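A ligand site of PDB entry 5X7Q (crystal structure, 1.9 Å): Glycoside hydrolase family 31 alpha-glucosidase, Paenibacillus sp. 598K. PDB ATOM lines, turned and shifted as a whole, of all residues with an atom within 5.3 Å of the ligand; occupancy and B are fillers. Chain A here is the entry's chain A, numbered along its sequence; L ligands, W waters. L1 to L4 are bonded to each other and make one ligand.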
ATOM      1  N   ARG A 344      -4.124   6.613 -23.470  1.00  0.00           N
ATOM      2  CA  ARG A 344      -4.795   5.939 -22.367  1.00  0.00           C
ATOM      3  C   ARG A 344      -6.279   6.198 -22.490  1.00  0.00           C
ATOM      4  O   ARG A 344      -6.673   7.374 -22.537  1.00  0.00           O
ATOM      5  CB  ARG A 344      -4.405   6.539 -21.010  1.00  0.00           C
ATOM      6  CG  ARG A 344      -2.968   6.380 -20.614  1.00  0.00           C
ATOM      7  CD  ARG A 344      -2.786   5.123 -19.800  1.00  0.00           C
ATOM      8  NE  ARG A 344      -1.411   4.999 -19.317  1.00  0.00           N
ATOM      9  CZ  ARG A 344      -0.936   3.917 -18.732  1.00  0.00           C
ATOM     10  NH1 ARG A 344      -1.723   2.845 -18.522  1.00  0.00           N
ATOM     11  NH2 ARG A 344       0.332   3.885 -18.347  1.00  0.00           N
ATOM     12  N   ASN A 348      -7.970   3.932 -18.249  1.00  0.00           N
ATOM     13  CA  ASN A 348      -6.512   3.890 -18.057  1.00  0.00           C
ATOM     14  C   ASN A 348      -5.745   2.746 -18.743  1.00  0.00           C
ATOM     15  O   ASN A 348      -4.636   2.376 -18.312  1.00  0.00           O
ATOM     16  CB  ASN A 348      -6.149   3.925 -16.559  1.00  0.00           C
ATOM     17  CG  ASN A 348      -4.745   4.461 -16.306  1.00  0.00           C
ATOM     18  OD1 ASN A 348      -4.386   5.515 -16.828  1.00  0.00           O
ATOM     19  ND2 ASN A 348      -3.952   3.724 -15.543  1.00  0.00           N
ATOM     20  N   ARG A 350      -3.739   1.251 -22.075  1.00  0.00           N
ATOM     21  CA  ARG A 350      -3.024   1.627 -23.293  1.00  0.00           C
ATOM     22  C   ARG A 350      -3.910   1.320 -24.512  1.00  0.00           C
ATOM     23  O   ARG A 350      -4.553   0.261 -24.575  1.00  0.00           O
ATOM     24  CB  ARG A 350      -1.693   0.878 -23.405  1.00  0.00           C
ATOM     25  CG  ARG A 350      -0.578   1.345 -22.465  1.00  0.00           C
ATOM     26  CD  ARG A 350      -0.457   2.843 -22.484  1.00  0.00           C
ATOM     27  NE  ARG A 350       0.815   3.367 -22.055  1.00  0.00           N
ATOM     28  CZ  ARG A 350       1.137   4.667 -22.125  1.00  0.00           C
ATOM     29  NH1 ARG A 350       0.246   5.556 -22.582  1.00  0.00           N
ATOM     30  NH2 ARG A 350       2.332   5.076 -21.714  1.00  0.00           N
ATOM     31  N   TYR A 354      -2.017   3.997 -29.581  1.00  0.00           N
ATOM     32  CA  TYR A 354      -0.741   4.150 -28.870  1.00  0.00           C
ATOM     33  C   TYR A 354       0.300   3.093 -29.296  1.00  0.00           C
ATOM     34  O   TYR A 354       1.422   3.433 -29.673  1.00  0.00           O
ATOM     35  CB  TYR A 354      -0.955   4.049 -27.357  1.00  0.00           C
ATOM     36  CG  TYR A 354       0.334   3.798 -26.616  1.00  0.00           C
ATOM     37  CD1 TYR A 354       1.255   4.832 -26.427  1.00  0.00           C
ATOM     38  CD2 TYR A 354       0.655   2.534 -26.100  1.00  0.00           C
ATOM     39  CE1 TYR A 354       2.430   4.619 -25.749  1.00  0.00           C
ATOM     40  CE2 TYR A 354       1.847   2.307 -25.445  1.00  0.00           C
ATOM     41  CZ  TYR A 354       2.733   3.352 -25.266  1.00  0.00           C
ATOM     42  OH  TYR A 354       3.924   3.165 -24.607  1.00  0.00           O
ATOM     43  N   TYR A 355      -0.104   1.824 -29.228  1.00  0.00           N
ATOM     44  CA  TYR A 355       0.793   0.725 -29.610  1.00  0.00           C
ATOM     45  C   TYR A 355       1.296   0.901 -31.030  1.00  0.00           C
ATOM     46  O   TYR A 355       2.496   0.734 -31.285  1.00  0.00           O
ATOM     47  CB  TYR A 355       0.122  -0.641 -29.450  1.00  0.00           C
ATOM     48  CG  TYR A 355      -0.079  -1.069 -28.008  1.00  0.00           C
ATOM     49  CD1 TYR A 355       0.981  -1.091 -27.097  1.00  0.00           C
ATOM     50  CD2 TYR A 355      -1.334  -1.477 -27.557  1.00  0.00           C
ATOM     51  CE1 TYR A 355       0.780  -1.491 -25.781  1.00  0.00           C
ATOM     52  CE2 TYR A 355      -1.543  -1.866 -26.240  1.00  0.00           C
ATOM     53  CZ  TYR A 355      -0.479  -1.885 -25.359  1.00  0.00           C
ATOM     54  OH  TYR A 355      -0.679  -2.277 -24.065  1.00  0.00           O
ATOM     55  N   ASP A 358       3.539   4.142 -31.231  1.00  0.00           N
ATOM     56  CA  ASP A 358       4.773   3.965 -30.465  1.00  0.00           C
ATOM     57  C   ASP A 358       5.724   3.007 -31.203  1.00  0.00           C
ATOM     58  O   ASP A 358       6.906   3.306 -31.392  1.00  0.00           O
ATOM     59  CB  ASP A 358       4.482   3.463 -29.043  1.00  0.00           C
ATOM     60  CG  ASP A 358       5.697   3.524 -28.125  1.00  0.00           C
ATOM     61  OD1 ASP A 358       6.253   4.617 -27.928  1.00  0.00           O
ATOM     62  OD2 ASP A 358       6.091   2.467 -27.607  1.00  0.00           O
ATOM     63  N   SER A1137      19.818  -2.150 -29.275  1.00  0.00           N
ATOM     64  CA  SER A1137      19.823  -2.797 -27.963  1.00  0.00           C
ATOM     65  C   SER A1137      18.415  -2.760 -27.363  1.00  0.00           C
ATOM     66  O   SER A1137      17.750  -1.749 -27.411  1.00  0.00           O
ATOM     67  CB  SER A1137      20.811  -2.126 -27.007  1.00  0.00           C
ATOM     68  OG  SER A1137      20.775  -2.765 -25.747  1.00  0.00           O
ATOM     69  N   ALA A1138      17.985  -3.902 -26.813  1.00  0.00           N
ATOM     70  CA  ALA A1138      16.735  -4.001 -26.069  1.00  0.00           C
ATOM     71  C   ALA A1138      16.945  -3.888 -24.544  1.00  0.00           C
ATOM     72  O   ALA A1138      15.977  -3.924 -23.770  1.00  0.00           O
ATOM     73  CB  ALA A1138      16.033  -5.303 -26.421  1.00  0.00           C
ATOM     74  N   PHE A1139      18.205  -3.724 -24.120  1.00  0.00           N
ATOM     75  CA  PHE A1139      18.622  -3.813 -22.728  1.00  0.00           C
ATOM     76  C   PHE A1139      18.841  -2.421 -22.126  1.00  0.00           C
ATOM     77  O   PHE A1139      19.414  -1.556 -22.775  1.00  0.00           O
ATOM     78  CB  PHE A1139      19.906  -4.654 -22.627  1.00  0.00           C
ATOM     79  CG  PHE A1139      20.724  -4.433 -21.366  1.00  0.00           C
ATOM     80  CD1 PHE A1139      20.204  -4.753 -20.101  1.00  0.00           C
ATOM     81  CD2 PHE A1139      22.021  -3.911 -21.438  1.00  0.00           C
ATOM     82  CE1 PHE A1139      20.967  -4.548 -18.958  1.00  0.00           C
ATOM     83  CE2 PHE A1139      22.776  -3.711 -20.293  1.00  0.00           C
ATOM     84  CZ  PHE A1139      22.248  -4.027 -19.050  1.00  0.00           C
ATOM     85  N   ASP A1142      16.974   0.572 -15.171  1.00  0.00           N
ATOM     86  CA  ASP A1142      16.318   1.695 -14.481  1.00  0.00           C
ATOM     87  C   ASP A1142      15.395   1.170 -13.370  1.00  0.00           C
ATOM     88  O   ASP A1142      15.423  -0.018 -13.062  1.00  0.00           O
ATOM     89  CB  ASP A1142      15.641   2.679 -15.461  1.00  0.00           C
ATOM     90  CG  ASP A1142      14.499   2.058 -16.265  1.00  0.00           C
ATOM     91  OD1 ASP A1142      13.631   1.341 -15.693  1.00  0.00           O
ATOM     92  OD2 ASP A1142      14.456   2.343 -17.491  1.00  0.00           O
ATOM     93  N   GLY A1144      11.861   1.512 -13.159  1.00  0.00           N
ATOM     94  CA  GLY A1144      10.472   1.197 -13.516  1.00  0.00           C
ATOM     95  C   GLY A1144       9.432   2.126 -12.926  1.00  0.00           C
ATOM     96  O   GLY A1144       8.225   1.831 -12.978  1.00  0.00           O
ATOM     97  N   LEU A1147       6.574   4.081 -15.160  1.00  0.00           N
ATOM     98  CA  LEU A1147       5.426   3.308 -15.594  1.00  0.00           C
ATOM     99  C   LEU A1147       4.262   3.437 -14.635  1.00  0.00           C
ATOM    100  O   LEU A1147       4.456   3.586 -13.436  1.00  0.00           O
ATOM    101  CB  LEU A1147       5.819   1.839 -15.727  1.00  0.00           C
ATOM    102  CG  LEU A1147       7.045   1.538 -16.586  1.00  0.00           C
ATOM    103  CD1 LEU A1147       7.564   0.128 -16.343  1.00  0.00           C
ATOM    104  CD2 LEU A1147       6.733   1.771 -18.062  1.00  0.00           C
ATOM    105  N   HIS A1148       3.047   3.346 -15.182  1.00  0.00           N
ATOM    106  CA  HIS A1148       1.817   3.385 -14.391  1.00  0.00           C
ATOM    107  C   HIS A1148       0.979   2.136 -14.659  1.00  0.00           C
ATOM    108  O   HIS A1148       0.457   2.011 -15.745  1.00  0.00           O
ATOM    109  CB  HIS A1148       1.030   4.633 -14.764  1.00  0.00           C
ATOM    110  CG  HIS A1148       1.744   5.893 -14.425  1.00  0.00           C
ATOM    111  ND1 HIS A1148       1.989   6.283 -13.121  1.00  0.00           N
ATOM    112  CD2 HIS A1148       2.298   6.849 -15.209  1.00  0.00           C
ATOM    113  CE1 HIS A1148       2.642   7.434 -13.128  1.00  0.00           C
ATOM    114  NE2 HIS A1148       2.835   7.794 -14.381  1.00  0.00           N
ATOM    115  N   PRO A1149       0.863   1.216 -13.674  1.00  0.00           N
ATOM    116  CA  PRO A1149       1.542   1.204 -12.358  1.00  0.00           C
ATOM    117  C   PRO A1149       3.054   0.916 -12.497  1.00  0.00           C
ATOM    118  O   PRO A1149       3.491   0.481 -13.563  1.00  0.00           O
ATOM    119  CB  PRO A1149       0.843   0.063 -11.608  1.00  0.00           C
ATOM    120  CG  PRO A1149       0.382  -0.855 -12.705  1.00  0.00           C
ATOM    121  CD  PRO A1149      -0.043   0.065 -13.818  1.00  0.00           C
ATOM    122  N   GLU A1151       6.621  -0.912 -12.472  1.00  0.00           N
ATOM    123  CA  GLU A1151       7.170  -2.248 -12.560  1.00  0.00           C
ATOM    124  C   GLU A1151       8.532  -2.173 -11.900  1.00  0.00           C
ATOM    125  O   GLU A1151       9.550  -2.005 -12.566  1.00  0.00           O
ATOM    126  CB  GLU A1151       7.257  -2.700 -14.010  1.00  0.00           C
ATOM    127  CG  GLU A1151       5.894  -2.809 -14.666  1.00  0.00           C
ATOM    128  CD  GLU A1151       5.972  -3.090 -16.153  1.00  0.00           C
ATOM    129  OE1 GLU A1151       7.024  -3.584 -16.637  1.00  0.00           O
ATOM    130  OE2 GLU A1151       4.984  -2.781 -16.852  1.00  0.00           O
ATOM    131  N   ARG A1159      16.687  -2.345 -11.634  1.00  0.00           N
ATOM    132  CA  ARG A1159      16.758  -3.703 -12.205  1.00  0.00           C
ATOM    133  C   ARG A1159      17.030  -3.590 -13.693  1.00  0.00           C
ATOM    134  O   ARG A1159      16.663  -2.589 -14.348  1.00  0.00           O
ATOM    135  CB  ARG A1159      15.477  -4.504 -11.905  1.00  0.00           C
ATOM    136  CG  ARG A1159      14.224  -4.104 -12.704  1.00  0.00           C
ATOM    137  CD  ARG A1159      13.660  -2.740 -12.350  1.00  0.00           C
ATOM    138  NE  ARG A1159      12.413  -2.421 -13.040  1.00  0.00           N
ATOM    139  CZ  ARG A1159      12.319  -2.000 -14.314  1.00  0.00           C
ATOM    140  NH1 ARG A1159      13.404  -1.814 -15.059  1.00  0.00           N
ATOM    141  NH2 ARG A1159      11.113  -1.734 -14.826  1.00  0.00           N
ATOM    142  N   TYR A1161      16.388  -4.517 -17.571  1.00  0.00           N
ATOM    143  CA  TYR A1161      15.241  -4.896 -18.405  1.00  0.00           C
ATOM    144  C   TYR A1161      15.707  -5.257 -19.802  1.00  0.00           C
ATOM    145  O   TYR A1161      16.678  -4.710 -20.303  1.00  0.00           O
ATOM    146  CB  TYR A1161      14.204  -3.771 -18.484  1.00  0.00           C
ATOM    147  CG  TYR A1161      14.678  -2.507 -19.177  1.00  0.00           C
ATOM    148  CD1 TYR A1161      14.577  -2.366 -20.573  1.00  0.00           C
ATOM    149  CD2 TYR A1161      15.199  -1.443 -18.452  1.00  0.00           C
ATOM    150  CE1 TYR A1161      15.020  -1.215 -21.199  1.00  0.00           C
ATOM    151  CE2 TYR A1161      15.639  -0.287 -19.070  1.00  0.00           C
ATOM    152  CZ  TYR A1161      15.548  -0.173 -20.451  1.00  0.00           C
ATOM    153  OH  TYR A1161      15.979   0.961 -21.066  1.00  0.00           O
ATOM    154  N   HIS A1163      13.543  -5.157 -23.317  1.00  0.00           N
ATOM    155  CA  HIS A1163      12.263  -4.836 -23.937  1.00  0.00           C
ATOM    156  C   HIS A1163      12.474  -4.226 -25.305  1.00  0.00           C
ATOM    157  O   HIS A1163      13.347  -3.386 -25.478  1.00  0.00           O
ATOM    158  CB  HIS A1163      11.436  -3.858 -23.086  1.00  0.00           C
ATOM    159  CG  HIS A1163      10.113  -3.522 -23.693  1.00  0.00           C
ATOM    160  ND1 HIS A1163       8.975  -4.240 -23.434  1.00  0.00           N
ATOM    161  CD2 HIS A1163       9.765  -2.572 -24.606  1.00  0.00           C
ATOM    162  CE1 HIS A1163       7.972  -3.739 -24.135  1.00  0.00           C
ATOM    163  NE2 HIS A1163       8.425  -2.732 -24.850  1.00  0.00           N
ATOM    164  N   SER A1164      11.672  -4.677 -26.258  1.00  0.00           N
ATOM    165  CA  SER A1164      11.491  -3.967 -27.523  1.00  0.00           C
ATOM    166  C   SER A1164      10.066  -4.161 -28.008  1.00  0.00           C
ATOM    167  O   SER A1164       9.457  -5.203 -27.732  1.00  0.00           O
ATOM    168  CB  SER A1164      12.461  -4.455 -28.585  1.00  0.00           C
ATOM    169  OG  SER A1164      12.178  -3.837 -29.815  1.00  0.00           O
ATOM    170  N   ASP A1165       9.559  -3.156 -28.732  1.00  0.00           N
ATOM    171  CA  ASP A1165       8.202  -3.170 -29.305  1.00  0.00           C
ATOM    172  C   ASP A1165       8.136  -4.102 -30.514  1.00  0.00           C
ATOM    173  O   ASP A1165       7.042  -4.496 -30.916  1.00  0.00           O
ATOM    174  CB  ASP A1165       7.748  -1.766 -29.747  1.00  0.00           C
ATOM    175  CG  ASP A1165       7.477  -0.797 -28.582  1.00  0.00           C
ATOM    176  OD1 ASP A1165       7.214  -1.236 -27.424  1.00  0.00           O
ATOM    177  OD2 ASP A1165       7.519   0.435 -28.835  1.00  0.00           O
ATOM    178  N   LYS A1194       6.851 -10.475 -18.419  1.00  0.00           N
ATOM    179  CA  LYS A1194       5.470 -10.105 -18.723  1.00  0.00           C
ATOM    180  C   LYS A1194       5.295  -9.767 -20.205  1.00  0.00           C
ATOM    181  O   LYS A1194       6.282  -9.719 -20.969  1.00  0.00           O
ATOM    182  CB  LYS A1194       4.992  -8.980 -17.797  1.00  0.00           C
ATOM    183  CG  LYS A1194       5.662  -7.632 -17.956  1.00  0.00           C
ATOM    184  CD  LYS A1194       5.758  -6.884 -16.619  1.00  0.00           C
ATOM    185  CE  LYS A1194       4.438  -6.658 -15.895  1.00  0.00           C
ATOM    186  NZ  LYS A1194       3.517  -5.710 -16.575  1.00  0.00           N
ATOM    187  N   ASN A1195       4.035  -9.596 -20.590  1.00  0.00           N
ATOM    188  CA  ASN A1195       3.635  -9.261 -21.952  1.00  0.00           C
ATOM    189  C   ASN A1195       3.853 -10.485 -22.865  1.00  0.00           C
ATOM    190  O   ASN A1195       3.513 -11.567 -22.438  1.00  0.00           O
ATOM    191  CB  ASN A1195       4.306  -7.974 -22.422  1.00  0.00           C
ATOM    192  CG  ASN A1195       4.032  -6.820 -21.478  1.00  0.00           C
ATOM    193  OD1 ASN A1195       2.891  -6.583 -21.097  1.00  0.00           O
ATOM    194  ND2 ASN A1195       5.083  -6.108 -21.107  1.00  0.00           N
ATOM    195  N   TYR A1249       7.655  -7.338 -28.030  1.00  0.00           N
ATOM    196  CA  TYR A1249       6.913  -6.933 -26.849  1.00  0.00           C
ATOM    197  C   TYR A1249       7.009  -7.914 -25.657  1.00  0.00           C
ATOM    198  O   TYR A1249       6.133  -7.926 -24.786  1.00  0.00           O
ATOM    199  CB  TYR A1249       5.447  -6.566 -27.210  1.00  0.00           C
ATOM    200  CG  TYR A1249       4.906  -5.387 -26.401  1.00  0.00           C
ATOM    201  CD1 TYR A1249       5.305  -4.085 -26.702  1.00  0.00           C
ATOM    202  CD2 TYR A1249       4.043  -5.580 -25.312  1.00  0.00           C
ATOM    203  CE1 TYR A1249       4.858  -2.997 -25.944  1.00  0.00           C
ATOM    204  CE2 TYR A1249       3.566  -4.502 -24.555  1.00  0.00           C
ATOM    205  CZ  TYR A1249       3.986  -3.202 -24.874  1.00  0.00           C
ATOM    206  OH  TYR A1249       3.550  -2.123 -24.146  1.00  0.00           O
ATOM    207  N   THR A1251       8.819  -8.416 -22.220  1.00  0.00           N
ATOM    208  CA  THR A1251       9.553  -7.700 -21.187  1.00  0.00           C
ATOM    209  C   THR A1251      10.149  -8.710 -20.212  1.00  0.00           C
ATOM    210  O   THR A1251       9.409  -9.479 -19.600  1.00  0.00           O
ATOM    211  CB  THR A1251       8.612  -6.752 -20.436  1.00  0.00           C
ATOM    212  OG1 THR A1251       7.974  -5.870 -21.377  1.00  0.00           O
ATOM    213  CG2 THR A1251       9.373  -5.942 -19.396  1.00  0.00           C
ATOM    214  N   HIS A1253      12.575  -8.666 -16.736  1.00  0.00           N
ATOM    215  CA  HIS A1253      13.338  -7.973 -15.699  1.00  0.00           C
ATOM    216  C   HIS A1253      14.237  -8.944 -14.975  1.00  0.00           C
ATOM    217  O   HIS A1253      13.850 -10.079 -14.686  1.00  0.00           O
ATOM    218  CB  HIS A1253      12.415  -7.244 -14.705  1.00  0.00           C
ATOM    219  CG  HIS A1253      11.527  -6.224 -15.356  1.00  0.00           C
ATOM    220  ND1 HIS A1253      10.163  -6.253 -15.248  1.00  0.00           N
ATOM    221  CD2 HIS A1253      11.825  -5.181 -16.162  1.00  0.00           C
ATOM    222  CE1 HIS A1253       9.647  -5.238 -15.928  1.00  0.00           C
ATOM    223  NE2 HIS A1253      10.639  -4.576 -16.487  1.00  0.00           N
HETATM  224  C1  LIG L   1       1.079  -0.856 -19.374  1.00  0.00           C
HETATM  225  C2  LIG L   1       2.433  -1.479 -19.610  1.00  0.00           C
HETATM  226  C3  LIG L   1       3.273  -0.532 -20.437  1.00  0.00           C
HETATM  227  C4  LIG L   1       3.217   0.955 -20.012  1.00  0.00           C
HETATM  228  C5  LIG L   1       3.802   1.842 -21.106  1.00  0.00           C
HETATM  229  C6  LIG L   1       1.371   0.464 -18.662  1.00  0.00           C
HETATM  230  O1  LIG L   1       0.190   1.000 -18.094  1.00  0.00           O
HETATM  231  O2  LIG L   1       0.240  -1.708 -18.592  1.00  0.00           O
HETATM  232  O3  LIG L   1       2.305  -2.745 -20.255  1.00  0.00           O
HETATM  233  O4  LIG L   1       4.621  -0.930 -20.247  1.00  0.00           O
HETATM  234  O5  LIG L   1       1.891   1.334 -19.663  1.00  0.00           O
HETATM  235  O6  LIG L   1       4.051   3.145 -20.565  1.00  0.00           O
HETATM  236  C1  LG2 L   2       5.152  -1.835 -21.219  1.00  0.00           C
HETATM  237  C2  LG2 L   2       5.908  -2.925 -20.451  1.00  0.00           C
HETATM  238  C3  LG2 L   2       7.139  -2.313 -19.749  1.00  0.00           C
HETATM  239  C4  LG2 L   2       7.975  -1.535 -20.747  1.00  0.00           C
HETATM  240  C5  LG2 L   2       7.154  -0.487 -21.499  1.00  0.00           C
HETATM  241  C6  LG2 L   2       7.967   0.194 -22.598  1.00  0.00           C
HETATM  242  O1  LG2 L   2       5.064  -3.523 -19.456  1.00  0.00           O
HETATM  243  O2  LG2 L   2       7.924  -3.339 -19.144  1.00  0.00           O
HETATM  244  O3  LG2 L   2       8.991  -0.859 -20.013  1.00  0.00           O
HETATM  245  O4  LG2 L   2       5.998  -1.086 -22.100  1.00  0.00           O
HETATM  246  O5  LG2 L   2       7.288   1.385 -22.978  1.00  0.00           O
HETATM  247  C1  LG3 L   3      10.318  -1.383 -20.196  1.00  0.00           C
HETATM  248  C2  LG3 L   3      11.030  -1.475 -18.849  1.00  0.00           C
HETATM  249  C3  LG3 L   3      11.322  -0.086 -18.302  1.00  0.00           C
HETATM  250  C4  LG3 L   3      12.100   0.715 -19.328  1.00  0.00           C
HETATM  251  C5  LG3 L   3      11.382   0.719 -20.680  1.00  0.00           C
HETATM  252  C6  LG3 L   3      12.244   1.347 -21.769  1.00  0.00           C
HETATM  253  O1  LG3 L   3      10.245  -2.220 -17.907  1.00  0.00           O
HETATM  254  O2  LG3 L   3      12.122  -0.228 -17.131  1.00  0.00           O
HETATM  255  O3  LG3 L   3      12.266   2.058 -18.870  1.00  0.00           O
HETATM  256  O4  LG3 L   3      11.088  -0.606 -21.117  1.00  0.00           O
HETATM  257  O5  LG3 L   3      11.370   1.852 -22.782  1.00  0.00           O
HETATM  258  C1  LG4 L   4      12.084   2.560 -23.816  1.00  0.00           C
HETATM  259  C2  LG4 L   4      11.039   3.197 -24.733  1.00  0.00           C
HETATM  260  C3  LG4 L   4      10.274   2.104 -25.492  1.00  0.00           C
HETATM  261  C4  LG4 L   4      11.265   1.170 -26.195  1.00  0.00           C
HETATM  262  C5  LG4 L   4      12.336   0.625 -25.228  1.00  0.00           C
HETATM  263  C6  LG4 L   4      13.400  -0.211 -25.925  1.00  0.00           C
HETATM  264  O1  LG4 L   4      10.122   3.983 -23.963  1.00  0.00           O
HETATM  265  O2  LG4 L   4       9.314   2.636 -26.435  1.00  0.00           O
HETATM  266  O3  LG4 L   4      10.512   0.082 -26.740  1.00  0.00           O
HETATM  267  O4  LG4 L   4      12.985   1.721 -24.542  1.00  0.00           O
HETATM  268  O5  LG4 L   4      14.174  -0.913 -24.947  1.00  0.00           O
HETATM  269  O   HOH W   1      10.293   3.398 -17.830  1.00  0.00           O
HETATM  270  O   HOH W   2       3.069   4.007 -18.052  1.00  0.00           O
HETATM  271  O   HOH W   3       4.606   0.488 -24.159  1.00  0.00           O
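N of Gly 1144 sits at hydrogen-bond distance from OD1 of Asp 1142, at 3.1 Å.
The backbone carbonyl oxygen (O) of Thr 1251 is in hydrogen-bond range of the backbone NH (N) of Lys 1194 (3.0 Å).
O of Ser 1164 is in hydrogen-bond range of N of Tyr 1249, 2.8 Å away.
A ring nitrogen (NE2) of His 1253 is in hydrogen-bond range of the guanidinium group of Arg 1159 (3.3 Å).
The backbone NH (N) of His 1163 lies within hydrogen-bond range of the backbone carbonyl oxygen (O) of Ala 1138, 2.8 Å away.
ND1 of His 1163 sits at hydrogen-bond distance from OG1 of Thr 1251, 2.8 Å away.
OE2 of Glu 1151 lies within salt-bridge range of NZ of Lys 1194 (3.3 Å).
The backbone carbonyl oxygen (O) of Gly 1144 is in hydrogen-bond range of the backbone NH (N) of Glu 1151 (3.2 Å).
Water W2 lies within hydrogen-bond range of NH2 of Arg 344 (2.8 Å), O6 of LIG L1 (2.8 Å) and N of His 1148 (2.9 Å).
Water W3 lies within hydrogen-bond range of the side-chain hydroxyl of Tyr 354 (2.8 Å), the side-chain hydroxyl of Tyr 1249 (2.8 Å) and an oxygen (O4) of LG2 L2 (2.9 Å).
Residues that only touch the ligand: Tyr 1161, Asp 1165, Ala 1138, Tyr 354, Leu 1147 and Lys 1194.
Hydrophobic or aromatic side chains within 4 Å of the ligand: Leu 1147, Tyr 1161, His 1163 and His 1253.
Of the 25 residues printed, 18 come within 4 Å of the ligand.
O4 of LG2 L2 lies close to OH of Tyr 1249 (3.4 Å).
The backbone carbonyl oxygen (O) of His 1148 lies within hydrogen-bond range of an oxygen (O1) of LIG L1.
O5 of LG4 L4 is in hydrogen-bond range of O of His 1163, 2.7 Å away.
The side-chain carboxylate of Asp 358 sits at hydrogen-bond distance from an oxygen (O2) of LG4 L4, at 3.4 Å.
ND2 of Asn 1195 is in hydrogen-bond range of O1 of LG2 L2 (3.1 Å).
O2 of LG2 L2 is in hydrogen-bond range of OE1 of Glu 1151, at 2.7 Å.
An oxygen (O3) of LG3 L3 lies within hydrogen-bond range of the side-chain carboxylate (OD2) of Asp 1142, at 2.6 Å.
NE2 of His 1253 sits at hydrogen-bond distance from O1 of LG3 L3 (2.8 Å).
OG1 of Thr 1251 sits close to O2 of LG2 L2.
An oxygen (O2) of LG3 L3 sits at hydrogen-bond distance from the guanidinium group of Arg 1159 (2.9 Å).
O6 of LIG L1 lies within hydrogen-bond range of NH2 of Arg 350.
O1 of LIG L1 is in hydrogen-bond range of NH1 of Arg 344, 2.7 Å away.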
